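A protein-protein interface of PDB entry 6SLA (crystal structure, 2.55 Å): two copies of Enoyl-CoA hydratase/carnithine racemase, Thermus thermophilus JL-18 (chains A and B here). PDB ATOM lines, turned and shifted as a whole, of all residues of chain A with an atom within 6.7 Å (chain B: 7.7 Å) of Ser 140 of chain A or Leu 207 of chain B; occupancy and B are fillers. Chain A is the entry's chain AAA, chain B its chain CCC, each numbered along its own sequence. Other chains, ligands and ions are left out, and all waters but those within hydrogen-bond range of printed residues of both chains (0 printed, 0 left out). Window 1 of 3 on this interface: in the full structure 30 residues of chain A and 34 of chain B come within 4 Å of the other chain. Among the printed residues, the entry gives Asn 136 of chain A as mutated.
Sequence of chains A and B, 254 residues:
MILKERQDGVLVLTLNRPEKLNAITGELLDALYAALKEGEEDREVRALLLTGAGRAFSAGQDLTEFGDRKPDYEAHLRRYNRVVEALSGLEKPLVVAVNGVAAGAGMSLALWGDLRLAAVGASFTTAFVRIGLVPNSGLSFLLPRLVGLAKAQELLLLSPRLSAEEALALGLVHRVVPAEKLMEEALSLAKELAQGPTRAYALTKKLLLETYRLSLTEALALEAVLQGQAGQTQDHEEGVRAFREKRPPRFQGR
OG of Ser 108 of chain A sits at hydrogen-bond distance from O of Asn 136 of chain A, 3.0 Å away. NH1 of Arg 145 of chain A sits at hydrogen-bond distance from O of Phe 141 of chain A, at 2.9 Å. The backbone carbonyl oxygen of Ala 200 of chain B is in hydrogen-bond range of the side-chain hydroxyl of Thr 204 of chain B.
NE2 of Gln 227 of chain B lies within hydrogen-bond range of O of Val 134 of chain A (2.7 Å). The side-chain amide nitrogen (NE2) of Gln 227 of chain B is in hydrogen-bond range of the side-chain amide oxygen (OD1) of Asn 136 of chain A, 2.8 Å away. N of Ser 137 of chain A lies within hydrogen-bond range of OE1 of Glu 223 of chain B (3.3 Å). The backbone NH (N) of Gly 138 of chain A lies within hydrogen-bond range of the side-chain carboxylate (OE1) of Glu 223 of chain B (2.9 Å). OE2 of Glu 223 of chain B lies within hydrogen-bond range of N of Leu 139 of chain A. The side-chain hydroxyl of Thr 211 of chain B sits at hydrogen-bond distance from the backbone carbonyl oxygen of Ser 140 of chain A, at 2.9 Å. The side-chain carboxylate (OE2) of Glu 223 of chain B sits at hydrogen-bond distance from the backbone NH (N) of Ser 140 of chain A. The backbone carbonyl oxygen (O) of Pro 144 of chain A lies close to the side-chain hydroxyl (OH) of Tyr 212 of chain B, 3.3 Å away. NH2 of Arg 145 of chain A lies within hydrogen-bond range of O of Thr 211 of chain B (2.8 Å). O of Tyr 212 of chain B sits at hydrogen-bond distance from NH2 of Arg 145 of chain A (3.4 Å). NH2 of Arg 145 of chain A lies within hydrogen-bond range of O of Leu 214 of chain B (3.4 Å).
Among the printed residues, pairs that only touch across the chains: Val 134 of chain A with Leu 203 of chain B, Val 134 of chain A with Thr 204 of chain B, Val 134 of chain A with Leu 207 of chain B, Pro 135 of chain A with Thr 204 of chain B, Pro 135 of chain A with Leu 207 of chain B, Pro 135 of chain A with Glu 223 of chain B, Asn 136 of chain A with Glu 223 of chain B, Gly 138 of chain A with Leu 220 of chain B, Ser 140 of chain A with Leu 207 of chain B, Phe 141 of chain A with Thr 211 of chain B, Phe 141 of chain A with Leu 214 of chain B, Phe 141 of chain A with Ala 219 of chain B, Phe 141 of chain A with Glu 223 of chain B, Pro 144 of chain A with Leu 208 of chain B, Pro 144 of chain A with Thr 211 of chain B and Leu 156 of chain A with Leu 208 of chain B.
Of the printed residues of chain B, Pro 144 of chain A touches Leu 208, Thr 211 and Tyr 212. Printed residues of chain A within 4 Å of Leu 203 of chain B: Val 134 (3.5 Å). Lys 206 of chain B touches none of the printed residues of chain A. Leu 207 of chain B touches three residues of chain A. Printed residues of chain A within 4 Å of Leu 208 of chain B: Pro 144 and Leu 156. Printed residues of chain A within 4 Å of Leu 220 of chain B: Gly 138. The nearest residue of chain B that does not touch Ser 140 of chain A is Leu 208 of chain B (4.5 Å).
No position is printed for both chains.
Hydrophobic or aromatic side chains of chain A that line the printed part of chain B: Val 134, Pro 135, Phe 141, Pro 144 and Leu 156. Of the 24 printed residues of chain B, 11 touch a printed residue of chain A. Printed residues of chain B that touch a printed residue of chain A: Leu 203, Thr 204, Leu 207, Leu 208, Thr 211, Tyr 212, Leu 214, Ala 219, Leu 220, Glu 223 and Gln 227. Hydrophobic or aromatic side chains of chain B within 4 Å of the printed part of chain A: Leu 203, Leu 207, Leu 208, Tyr 212, Ala 219 and Leu 220. Among the printed residues, no Asp or Glu carboxylate lies within 4 Å of a Lys or Arg side-chain nitrogen of the other chain.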
ATOM      1  N   SER A 108     -19.239  -0.954 -22.302  1.00  0.00           N
ATOM      2  CA  SER A 108     -20.438  -0.158 -22.045  1.00  0.00           C
ATOM      3  C   SER A 108     -21.390  -0.905 -21.124  1.00  0.00           C
ATOM      4  O   SER A 108     -21.800  -0.357 -20.111  1.00  0.00           O
ATOM      5  CB  SER A 108     -21.154   0.291 -23.299  1.00  0.00           C
ATOM      6  OG  SER A 108     -20.231   0.849 -24.243  1.00  0.00           O
ATOM      7  N   VAL A 134     -17.064   5.644 -32.951  1.00  0.00           N
ATOM      8  CA  VAL A 134     -17.216   6.430 -31.734  1.00  0.00           C
ATOM      9  C   VAL A 134     -17.809   5.536 -30.647  1.00  0.00           C
ATOM     10  O   VAL A 134     -18.315   4.457 -30.947  1.00  0.00           O
ATOM     11  CB  VAL A 134     -18.078   7.681 -31.988  1.00  0.00           C
ATOM     12  CG1 VAL A 134     -17.532   8.469 -33.161  1.00  0.00           C
ATOM     13  CG2 VAL A 134     -19.554   7.345 -32.163  1.00  0.00           C
ATOM     14  N   PRO A 135     -17.764   5.929 -29.349  1.00  0.00           N
ATOM     15  CA  PRO A 135     -18.345   5.091 -28.297  1.00  0.00           C
ATOM     16  C   PRO A 135     -19.870   5.049 -28.429  1.00  0.00           C
ATOM     17  O   PRO A 135     -20.499   6.028 -28.810  1.00  0.00           O
ATOM     18  CB  PRO A 135     -17.933   5.763 -26.979  1.00  0.00           C
ATOM     19  CG  PRO A 135     -17.007   6.893 -27.363  1.00  0.00           C
ATOM     20  CD  PRO A 135     -17.200   7.179 -28.831  1.00  0.00           C
ATOM     21  N   ASN A 136     -20.449   3.930 -28.030  1.00  0.00           N
ATOM     22  CA  ASN A 136     -21.842   3.590 -28.181  1.00  0.00           C
ATOM     23  C   ASN A 136     -22.408   3.072 -26.860  1.00  0.00           C
ATOM     24  O   ASN A 136     -21.648   2.850 -25.922  1.00  0.00           O
ATOM     25  CB  ASN A 136     -21.862   2.367 -29.090  1.00  0.00           C
ATOM     26  CG  ASN A 136     -22.398   2.630 -30.466  1.00  0.00           C
ATOM     27  OD1 ASN A 136     -22.439   3.772 -30.930  1.00  0.00           O
ATOM     28  ND2 ASN A 136     -22.831   1.563 -31.108  1.00  0.00           N
ATOM     29  N   SER A 137     -23.723   2.794 -26.832  1.00  0.00           N
ATOM     30  CA  SER A 137     -24.319   2.046 -25.725  1.00  0.00           C
ATOM     31  C   SER A 137     -24.083   2.779 -24.408  1.00  0.00           C
ATOM     32  O   SER A 137     -23.989   2.155 -23.365  1.00  0.00           O
ATOM     33  CB  SER A 137     -23.790   0.622 -25.640  1.00  0.00           C
ATOM     34  OG  SER A 137     -23.997  -0.093 -26.858  1.00  0.00           O
ATOM     35  N   GLY A 138     -23.951   4.103 -24.474  1.00  0.00           N
ATOM     36  CA  GLY A 138     -23.925   4.936 -23.288  1.00  0.00           C
ATOM     37  C   GLY A 138     -22.511   5.259 -22.818  1.00  0.00           C
ATOM     38  O   GLY A 138     -22.374   5.968 -21.842  1.00  0.00           O
ATOM     39  N   LEU A 139     -21.466   4.788 -23.505  1.00  0.00           N
ATOM     40  CA  LEU A 139     -20.128   4.929 -22.945  1.00  0.00           C
ATOM     41  C   LEU A 139     -19.687   6.389 -22.923  1.00  0.00           C
ATOM     42  O   LEU A 139     -18.990   6.798 -21.998  1.00  0.00           O
ATOM     43  CB  LEU A 139     -19.116   4.086 -23.716  1.00  0.00           C
ATOM     44  CG  LEU A 139     -17.762   3.937 -23.022  1.00  0.00           C
ATOM     45  CD1 LEU A 139     -17.898   3.501 -21.539  1.00  0.00           C
ATOM     46  CD2 LEU A 139     -16.856   2.998 -23.833  1.00  0.00           C
ATOM     47  N   SER A 140     -20.100   7.171 -23.919  1.00  0.00           N
ATOM     48  CA  SER A 140     -19.734   8.581 -23.974  1.00  0.00           C
ATOM     49  C   SER A 140     -20.427   9.331 -22.841  1.00  0.00           C
ATOM     50  O   SER A 140     -19.918  10.346 -22.377  1.00  0.00           O
ATOM     51  CB  SER A 140     -20.029   9.222 -25.328  1.00  0.00           C
ATOM     52  OG  SER A 140     -21.429   9.423 -25.497  1.00  0.00           O
ATOM     53  N   PHE A 141     -21.560   8.793 -22.381  1.00  0.00           N
ATOM     54  CA  PHE A 141     -22.279   9.289 -21.215  1.00  0.00           C
ATOM     55  C   PHE A 141     -21.575   8.848 -19.931  1.00  0.00           C
ATOM     56  O   PHE A 141     -21.203   9.695 -19.113  1.00  0.00           O
ATOM     57  CB  PHE A 141     -23.744   8.831 -21.242  1.00  0.00           C
ATOM     58  CG  PHE A 141     -24.647   9.396 -20.166  1.00  0.00           C
ATOM     59  CD1 PHE A 141     -25.332  10.597 -20.386  1.00  0.00           C
ATOM     60  CD2 PHE A 141     -24.909   8.695 -18.995  1.00  0.00           C
ATOM     61  CE1 PHE A 141     -26.204  11.117 -19.452  1.00  0.00           C
ATOM     62  CE2 PHE A 141     -25.798   9.216 -18.054  1.00  0.00           C
ATOM     63  CZ  PHE A 141     -26.427  10.438 -18.273  1.00  0.00           C
ATOM     64  N   LEU A 142     -21.412   7.526 -19.753  1.00  0.00           N
ATOM     65  CA  LEU A 142     -20.986   6.948 -18.478  1.00  0.00           C
ATOM     66  C   LEU A 142     -19.531   7.301 -18.159  1.00  0.00           C
ATOM     67  O   LEU A 142     -19.218   7.678 -17.035  1.00  0.00           O
ATOM     68  CB  LEU A 142     -21.135   5.426 -18.532  1.00  0.00           C
ATOM     69  CG  LEU A 142     -22.393   4.864 -17.880  1.00  0.00           C
ATOM     70  CD1 LEU A 142     -22.367   3.354 -17.797  1.00  0.00           C
ATOM     71  CD2 LEU A 142     -22.601   5.422 -16.489  1.00  0.00           C
ATOM     72  N   LEU A 143     -18.646   7.154 -19.154  1.00  0.00           N
ATOM     73  CA  LEU A 143     -17.218   7.124 -18.874  1.00  0.00           C
ATOM     74  C   LEU A 143     -16.742   8.438 -18.252  1.00  0.00           C
ATOM     75  O   LEU A 143     -16.093   8.412 -17.204  1.00  0.00           O
ATOM     76  CB  LEU A 143     -16.412   6.752 -20.120  1.00  0.00           C
ATOM     77  CG  LEU A 143     -14.984   6.316 -19.818  1.00  0.00           C
ATOM     78  CD1 LEU A 143     -14.930   5.143 -18.804  1.00  0.00           C
ATOM     79  CD2 LEU A 143     -14.220   6.044 -21.123  1.00  0.00           C
ATOM     80  N   PRO A 144     -17.021   9.621 -18.859  1.00  0.00           N
ATOM     81  CA  PRO A 144     -16.552  10.889 -18.295  1.00  0.00           C
ATOM     82  C   PRO A 144     -17.143  11.105 -16.904  1.00  0.00           C
ATOM     83  O   PRO A 144     -16.464  11.650 -16.044  1.00  0.00           O
ATOM     84  CB  PRO A 144     -17.023  11.971 -19.263  1.00  0.00           C
ATOM     85  CG  PRO A 144     -17.413  11.195 -20.516  1.00  0.00           C
ATOM     86  CD  PRO A 144     -17.818   9.808 -20.087  1.00  0.00           C
ATOM     87  N   ARG A 145     -18.394  10.679 -16.684  1.00  0.00           N
ATOM     88  CA  ARG A 145     -19.003  10.752 -15.360  1.00  0.00           C
ATOM     89  C   ARG A 145     -18.256   9.862 -14.354  1.00  0.00           C
ATOM     90  O   ARG A 145     -18.033  10.262 -13.217  1.00  0.00           O
ATOM     91  CB  ARG A 145     -20.488  10.396 -15.401  1.00  0.00           C
ATOM     92  CG  ARG A 145     -21.310  11.380 -16.209  1.00  0.00           C
ATOM     93  CD  ARG A 145     -22.730  10.925 -16.523  1.00  0.00           C
ATOM     94  NE  ARG A 145     -23.618  12.016 -16.919  1.00  0.00           N
ATOM     95  CZ  ARG A 145     -23.530  12.627 -18.126  1.00  0.00           C
ATOM     96  NH1 ARG A 145     -22.580  12.278 -18.977  1.00  0.00           N
ATOM     97  NH2 ARG A 145     -24.338  13.608 -18.500  1.00  0.00           N
ATOM     98  N   LEU A 156     -10.579   6.639 -24.260  1.00  0.00           N
ATOM     99  CA  LEU A 156     -11.326   6.582 -25.512  1.00  0.00           C
ATOM    100  C   LEU A 156     -10.421   6.775 -26.735  1.00  0.00           C
ATOM    101  O   LEU A 156     -10.544   6.027 -27.713  1.00  0.00           O
ATOM    102  CB  LEU A 156     -12.461   7.609 -25.484  1.00  0.00           C
ATOM    103  CG  LEU A 156     -13.611   7.226 -24.567  1.00  0.00           C
ATOM    104  CD1 LEU A 156     -14.609   8.383 -24.443  1.00  0.00           C
ATOM    105  CD2 LEU A 156     -14.307   5.985 -25.082  1.00  0.00           C
ATOM    106  N   ALA B 200     -13.107   9.506 -36.461  1.00  0.00           N
ATOM    107  CA  ALA B 200     -13.496   8.913 -35.184  1.00  0.00           C
ATOM    108  C   ALA B 200     -13.056   9.825 -34.042  1.00  0.00           C
ATOM    109  O   ALA B 200     -13.824  10.069 -33.118  1.00  0.00           O
ATOM    110  CB  ALA B 200     -12.962   7.511 -35.012  1.00  0.00           C
ATOM    111  N   TYR B 201     -11.826  10.352 -34.135  1.00  0.00           N
ATOM    112  CA  TYR B 201     -11.329  11.296 -33.147  1.00  0.00           C
ATOM    113  C   TYR B 201     -12.266  12.503 -33.047  1.00  0.00           C
ATOM    114  O   TYR B 201     -12.716  12.837 -31.956  1.00  0.00           O
ATOM    115  CB  TYR B 201      -9.884  11.717 -33.431  1.00  0.00           C
ATOM    116  CG  TYR B 201      -8.850  10.625 -33.354  1.00  0.00           C
ATOM    117  CD1 TYR B 201      -8.955   9.592 -32.437  1.00  0.00           C
ATOM    118  CD2 TYR B 201      -7.708  10.667 -34.147  1.00  0.00           C
ATOM    119  CE1 TYR B 201      -7.987   8.602 -32.340  1.00  0.00           C
ATOM    120  CE2 TYR B 201      -6.733   9.687 -34.072  1.00  0.00           C
ATOM    121  CZ  TYR B 201      -6.876   8.651 -33.165  1.00  0.00           C
ATOM    122  OH  TYR B 201      -5.920   7.679 -33.073  1.00  0.00           O
ATOM    123  N   ALA B 202     -12.567  13.139 -34.184  1.00  0.00           N
ATOM    124  CA  ALA B 202     -13.367  14.357 -34.210  1.00  0.00           C
ATOM    125  C   ALA B 202     -14.722  14.137 -33.555  1.00  0.00           C
ATOM    126  O   ALA B 202     -15.155  14.977 -32.758  1.00  0.00           O
ATOM    127  CB  ALA B 202     -13.546  14.860 -35.620  1.00  0.00           C
ATOM    128  N   LEU B 203     -15.369  13.013 -33.893  1.00  0.00           N
ATOM    129  CA  LEU B 203     -16.739  12.789 -33.454  1.00  0.00           C
ATOM    130  C   LEU B 203     -16.803  12.372 -31.979  1.00  0.00           C
ATOM    131  O   LEU B 203     -17.744  12.741 -31.259  1.00  0.00           O
ATOM    132  CB  LEU B 203     -17.415  11.770 -34.387  1.00  0.00           C
ATOM    133  CG  LEU B 203     -17.596  12.222 -35.838  1.00  0.00           C
ATOM    134  CD1 LEU B 203     -18.218  11.118 -36.676  1.00  0.00           C
ATOM    135  CD2 LEU B 203     -18.434  13.484 -35.930  1.00  0.00           C
ATOM    136  N   THR B 204     -15.793  11.604 -31.532  1.00  0.00           N
ATOM    137  CA  THR B 204     -15.628  11.291 -30.122  1.00  0.00           C
ATOM    138  C   THR B 204     -15.505  12.581 -29.309  1.00  0.00           C
ATOM    139  O   THR B 204     -16.086  12.683 -28.231  1.00  0.00           O
ATOM    140  CB  THR B 204     -14.438  10.352 -29.901  1.00  0.00           C
ATOM    141  OG1 THR B 204     -14.695   9.189 -30.690  1.00  0.00           O
ATOM    142  CG2 THR B 204     -14.265   9.943 -28.459  1.00  0.00           C
ATOM    143  N   LYS B 205     -14.766  13.567 -29.833  1.00  0.00           N
ATOM    144  CA  LYS B 205     -14.583  14.826 -29.125  1.00  0.00           C
ATOM    145  C   LYS B 205     -15.907  15.578 -29.035  1.00  0.00           C
ATOM    146  O   LYS B 205     -16.170  16.219 -28.029  1.00  0.00           O
ATOM    147  CB  LYS B 205     -13.545  15.724 -29.797  1.00  0.00           C
ATOM    148  CG  LYS B 205     -12.106  15.265 -29.654  1.00  0.00           C
ATOM    149  CD  LYS B 205     -11.121  16.012 -30.541  1.00  0.00           C
ATOM    150  CE  LYS B 205     -11.185  17.510 -30.346  1.00  0.00           C
ATOM    151  NZ  LYS B 205      -9.910  18.137 -30.759  1.00  0.00           N
ATOM    152  N   LYS B 206     -16.737  15.509 -30.084  1.00  0.00           N
ATOM    153  CA  LYS B 206     -18.021  16.189 -30.083  1.00  0.00           C
ATOM    154  C   LYS B 206     -18.894  15.569 -28.992  1.00  0.00           C
ATOM    155  O   LYS B 206     -19.577  16.295 -28.281  1.00  0.00           O
ATOM    156  CB  LYS B 206     -18.631  16.221 -31.493  1.00  0.00           C
ATOM    157  CG  LYS B 206     -20.102  16.575 -31.627  1.00  0.00           C
ATOM    158  CD  LYS B 206     -20.358  18.065 -31.765  1.00  0.00           C
ATOM    159  CE  LYS B 206     -21.801  18.481 -31.522  1.00  0.00           C
ATOM    160  NZ  LYS B 206     -22.136  18.597 -30.075  1.00  0.00           N
ATOM    161  N   LEU B 207     -18.840  14.240 -28.829  1.00  0.00           N
ATOM    162  CA  LEU B 207     -19.593  13.575 -27.763  1.00  0.00           C
ATOM    163  C   LEU B 207     -19.110  14.015 -26.382  1.00  0.00           C
ATOM    164  O   LEU B 207     -19.921  14.289 -25.511  1.00  0.00           O
ATOM    165  CB  LEU B 207     -19.499  12.052 -27.920  1.00  0.00           C
ATOM    166  CG  LEU B 207     -20.250  11.456 -29.119  1.00  0.00           C
ATOM    167  CD1 LEU B 207     -19.791  10.025 -29.381  1.00  0.00           C
ATOM    168  CD2 LEU B 207     -21.786  11.503 -28.915  1.00  0.00           C
ATOM    169  N   LEU B 208     -17.789  14.108 -26.195  1.00  0.00           N
ATOM    170  CA  LEU B 208     -17.233  14.463 -24.895  1.00  0.00           C
ATOM    171  C   LEU B 208     -17.605  15.894 -24.530  1.00  0.00           C
ATOM    172  O   LEU B 208     -17.945  16.181 -23.377  1.00  0.00           O
ATOM    173  CB  LEU B 208     -15.713  14.243 -24.870  1.00  0.00           C
ATOM    174  CG  LEU B 208     -15.314  12.764 -24.977  1.00  0.00           C
ATOM    175  CD1 LEU B 208     -13.814  12.610 -25.008  1.00  0.00           C
ATOM    176  CD2 LEU B 208     -15.918  11.936 -23.851  1.00  0.00           C
ATOM    177  N   LEU B 209     -17.577  16.776 -25.525  1.00  0.00           N
ATOM    178  CA  LEU B 209     -17.867  18.179 -25.294  1.00  0.00           C
ATOM    179  C   LEU B 209     -19.307  18.360 -24.800  1.00  0.00           C
ATOM    180  O   LEU B 209     -19.565  19.282 -24.027  1.00  0.00           O
ATOM    181  CB  LEU B 209     -17.624  18.913 -26.613  1.00  0.00           C
ATOM    182  CG  LEU B 209     -17.488  20.414 -26.437  1.00  0.00           C
ATOM    183  CD1 LEU B 209     -16.152  20.741 -25.772  1.00  0.00           C
ATOM    184  CD2 LEU B 209     -17.762  21.157 -27.738  1.00  0.00           C
ATOM    185  N   GLU B 210     -20.228  17.466 -25.197  1.00  0.00           N
ATOM    186  CA  GLU B 210     -21.649  17.691 -24.949  1.00  0.00           C
ATOM    187  C   GLU B 210     -22.164  16.873 -23.757  1.00  0.00           C
ATOM    188  O   GLU B 210     -23.281  17.126 -23.255  1.00  0.00           O
ATOM    189  CB  GLU B 210     -22.504  17.276 -26.148  1.00  0.00           C
ATOM    190  CG  GLU B 210     -22.432  18.268 -27.296  1.00  0.00           C
ATOM    191  CD  GLU B 210     -23.015  19.653 -27.011  1.00  0.00           C
ATOM    192  OE1 GLU B 210     -23.841  19.819 -26.063  1.00  0.00           O
ATOM    193  OE2 GLU B 210     -22.655  20.594 -27.753  1.00  0.00           O
ATOM    194  N   THR B 211     -21.366  15.895 -23.311  1.00  0.00           N
ATOM    195  CA  THR B 211     -21.937  14.778 -22.578  1.00  0.00           C
ATOM    196  C   THR B 211     -22.652  15.215 -21.300  1.00  0.00           C
ATOM    197  O   THR B 211     -23.693  14.659 -20.978  1.00  0.00           O
ATOM    198  CB  THR B 211     -20.889  13.681 -22.318  1.00  0.00           C
ATOM    199  OG1 THR B 211     -21.691  12.602 -21.842  1.00  0.00           O
ATOM    200  CG2 THR B 211     -19.792  14.076 -21.347  1.00  0.00           C
ATOM    201  N   TYR B 212     -22.085  16.185 -20.568  1.00  0.00           N
ATOM    202  CA  TYR B 212     -22.499  16.511 -19.218  1.00  0.00           C
ATOM    203  C   TYR B 212     -23.873  17.164 -19.165  1.00  0.00           C
ATOM    204  O   TYR B 212     -24.572  17.009 -18.164  1.00  0.00           O
ATOM    205  CB  TYR B 212     -21.463  17.363 -18.477  1.00  0.00           C
ATOM    206  CG  TYR B 212     -20.182  16.637 -18.160  1.00  0.00           C
ATOM    207  CD1 TYR B 212     -20.064  15.797 -17.044  1.00  0.00           C
ATOM    208  CD2 TYR B 212     -19.086  16.767 -18.992  1.00  0.00           C
ATOM    209  CE1 TYR B 212     -18.894  15.114 -16.778  1.00  0.00           C
ATOM    210  CE2 TYR B 212     -17.914  16.077 -18.736  1.00  0.00           C
ATOM    211  CZ  TYR B 212     -17.815  15.256 -17.635  1.00  0.00           C
ATOM    212  OH  TYR B 212     -16.612  14.642 -17.417  1.00  0.00           O
ATOM    213  N   LEU B 214     -26.389  16.545 -21.266  1.00  0.00           N
ATOM    214  CA  LEU B 214     -27.375  15.714 -21.952  1.00  0.00           C
ATOM    215  C   LEU B 214     -27.965  14.669 -21.005  1.00  0.00           C
ATOM    216  O   LEU B 214     -27.276  14.126 -20.145  1.00  0.00           O
ATOM    217  CB  LEU B 214     -26.713  14.998 -23.130  1.00  0.00           C
ATOM    218  CG  LEU B 214     -26.222  15.845 -24.306  1.00  0.00           C
ATOM    219  CD1 LEU B 214     -25.802  14.896 -25.442  1.00  0.00           C
ATOM    220  CD2 LEU B 214     -27.256  16.889 -24.754  1.00  0.00           C
ATOM    221  N   GLU B 218     -30.882  11.615 -24.741  1.00  0.00           N
ATOM    222  CA  GLU B 218     -30.280  12.438 -25.778  1.00  0.00           C
ATOM    223  C   GLU B 218     -28.858  11.956 -26.081  1.00  0.00           C
ATOM    224  O   GLU B 218     -28.440  11.966 -27.252  1.00  0.00           O
ATOM    225  CB  GLU B 218     -30.285  13.926 -25.447  1.00  0.00           C
ATOM    226  CG  GLU B 218     -31.645  14.535 -25.149  1.00  0.00           C
ATOM    227  CD  GLU B 218     -31.540  15.830 -24.334  1.00  0.00           C
ATOM    228  OE1 GLU B 218     -30.836  15.833 -23.314  1.00  0.00           O
ATOM    229  OE2 GLU B 218     -32.160  16.869 -24.704  1.00  0.00           O
ATOM    230  N   ALA B 219     -28.133  11.501 -25.045  1.00  0.00           N
ATOM    231  CA  ALA B 219     -26.778  11.018 -25.289  1.00  0.00           C
ATOM    232  C   ALA B 219     -26.813   9.807 -26.238  1.00  0.00           C
ATOM    233  O   ALA B 219     -26.041   9.735 -27.199  1.00  0.00           O
ATOM    234  CB  ALA B 219     -26.059  10.743 -23.984  1.00  0.00           C
ATOM    235  N   LEU B 220     -27.747   8.872 -25.980  1.00  0.00           N
ATOM    236  CA  LEU B 220     -27.914   7.699 -26.837  1.00  0.00           C
ATOM    237  C   LEU B 220     -28.286   8.119 -28.261  1.00  0.00           C
ATOM    238  O   LEU B 220     -27.778   7.548 -29.225  1.00  0.00           O
ATOM    239  CB  LEU B 220     -28.960   6.753 -26.248  1.00  0.00           C
ATOM    240  CG  LEU B 220     -28.622   6.131 -24.892  1.00  0.00           C
ATOM    241  CD1 LEU B 220     -29.763   5.265 -24.373  1.00  0.00           C
ATOM    242  CD2 LEU B 220     -27.351   5.305 -24.954  1.00  0.00           C
ATOM    243  N   ALA B 221     -29.137   9.143 -28.402  1.00  0.00           N
ATOM    244  CA  ALA B 221     -29.548   9.569 -29.737  1.00  0.00           C
ATOM    245  C   ALA B 221     -28.350  10.159 -30.492  1.00  0.00           C
ATOM    246  O   ALA B 221     -28.133   9.848 -31.660  1.00  0.00           O
ATOM    247  CB  ALA B 221     -30.735  10.525 -29.683  1.00  0.00           C
ATOM    248  N   LEU B 222     -27.541  10.984 -29.817  1.00  0.00           N
ATOM    249  CA  LEU B 222     -26.413  11.602 -30.490  1.00  0.00           C
ATOM    250  C   LEU B 222     -25.365  10.550 -30.853  1.00  0.00           C
ATOM    251  O   LEU B 222     -24.802  10.601 -31.938  1.00  0.00           O
ATOM    252  CB  LEU B 222     -25.824  12.706 -29.604  1.00  0.00           C
ATOM    253  CG  LEU B 222     -24.712  13.537 -30.235  1.00  0.00           C
ATOM    254  CD1 LEU B 222     -25.270  14.290 -31.436  1.00  0.00           C
ATOM    255  CD2 LEU B 222     -24.138  14.498 -29.187  1.00  0.00           C
ATOM    256  N   GLU B 223     -25.132   9.578 -29.974  1.00  0.00           N
ATOM    257  CA  GLU B 223     -24.214   8.484 -30.266  1.00  0.00           C
ATOM    258  C   GLU B 223     -24.688   7.780 -31.544  1.00  0.00           C
ATOM    259  O   GLU B 223     -23.874   7.501 -32.432  1.00  0.00           O
ATOM    260  CB  GLU B 223     -24.113   7.497 -29.089  1.00  0.00           C
ATOM    261  CG  GLU B 223     -23.302   7.984 -27.895  1.00  0.00           C
ATOM    262  CD  GLU B 223     -23.169   7.026 -26.703  1.00  0.00           C
ATOM    263  OE1 GLU B 223     -23.998   6.102 -26.590  1.00  0.00           O
ATOM    264  OE2 GLU B 223     -22.252   7.213 -25.861  1.00  0.00           O
ATOM    265  N   ALA B 224     -26.007   7.514 -31.651  1.00  0.00           N
ATOM    266  CA  ALA B 224     -26.551   6.882 -32.846  1.00  0.00           C
ATOM    267  C   ALA B 224     -26.263   7.735 -34.084  1.00  0.00           C
ATOM    268  O   ALA B 224     -25.753   7.231 -35.073  1.00  0.00           O
ATOM    269  CB  ALA B 224     -28.016   6.597 -32.716  1.00  0.00           C
ATOM    270  N   VAL B 225     -26.555   9.039 -34.026  1.00  0.00           N
ATOM    271  CA  VAL B 225     -26.389   9.861 -35.208  1.00  0.00           C
ATOM    272  C   VAL B 225     -24.918   9.855 -35.607  1.00  0.00           C
ATOM    273  O   VAL B 225     -24.603   9.637 -36.770  1.00  0.00           O
ATOM    274  CB  VAL B 225     -26.924  11.290 -34.981  1.00  0.00           C
ATOM    275  CG1 VAL B 225     -26.426  12.269 -36.048  1.00  0.00           C
ATOM    276  CG2 VAL B 225     -28.443  11.338 -34.872  1.00  0.00           C
ATOM    277  N   LEU B 226     -24.012  10.081 -34.647  1.00  0.00           N
ATOM    278  CA  LEU B 226     -22.604  10.244 -34.982  1.00  0.00           C
ATOM    279  C   LEU B 226     -21.983   8.884 -35.312  1.00  0.00           C
ATOM    280  O   LEU B 226     -21.089   8.803 -36.135  1.00  0.00           O
ATOM    281  CB  LEU B 226     -21.836  10.957 -33.859  1.00  0.00           C
ATOM    282  CG  LEU B 226     -22.306  12.350 -33.427  1.00  0.00           C
ATOM    283  CD1 LEU B 226     -21.287  12.972 -32.482  1.00  0.00           C
ATOM    284  CD2 LEU B 226     -22.578  13.272 -34.602  1.00  0.00           C
ATOM    285  N   GLN B 227     -22.466   7.805 -34.700  1.00  0.00           N
ATOM    286  CA  GLN B 227     -22.012   6.471 -35.063  1.00  0.00           C
ATOM    287  C   GLN B 227     -22.422   6.160 -36.493  1.00  0.00           C
ATOM    288  O   GLN B 227     -21.659   5.540 -37.223  1.00  0.00           O
ATOM    289  CB  GLN B 227     -22.574   5.399 -34.121  1.00  0.00           C
ATOM    290  CG  GLN B 227     -21.854   4.066 -34.225  1.00  0.00           C
ATOM    291  CD  GLN B 227     -20.450   4.135 -33.674  1.00  0.00           C
ATOM    292  OE1 GLN B 227     -19.594   4.792 -34.233  1.00  0.00           O
ATOM    293  NE2 GLN B 227     -20.183   3.417 -32.592  1.00  0.00           N
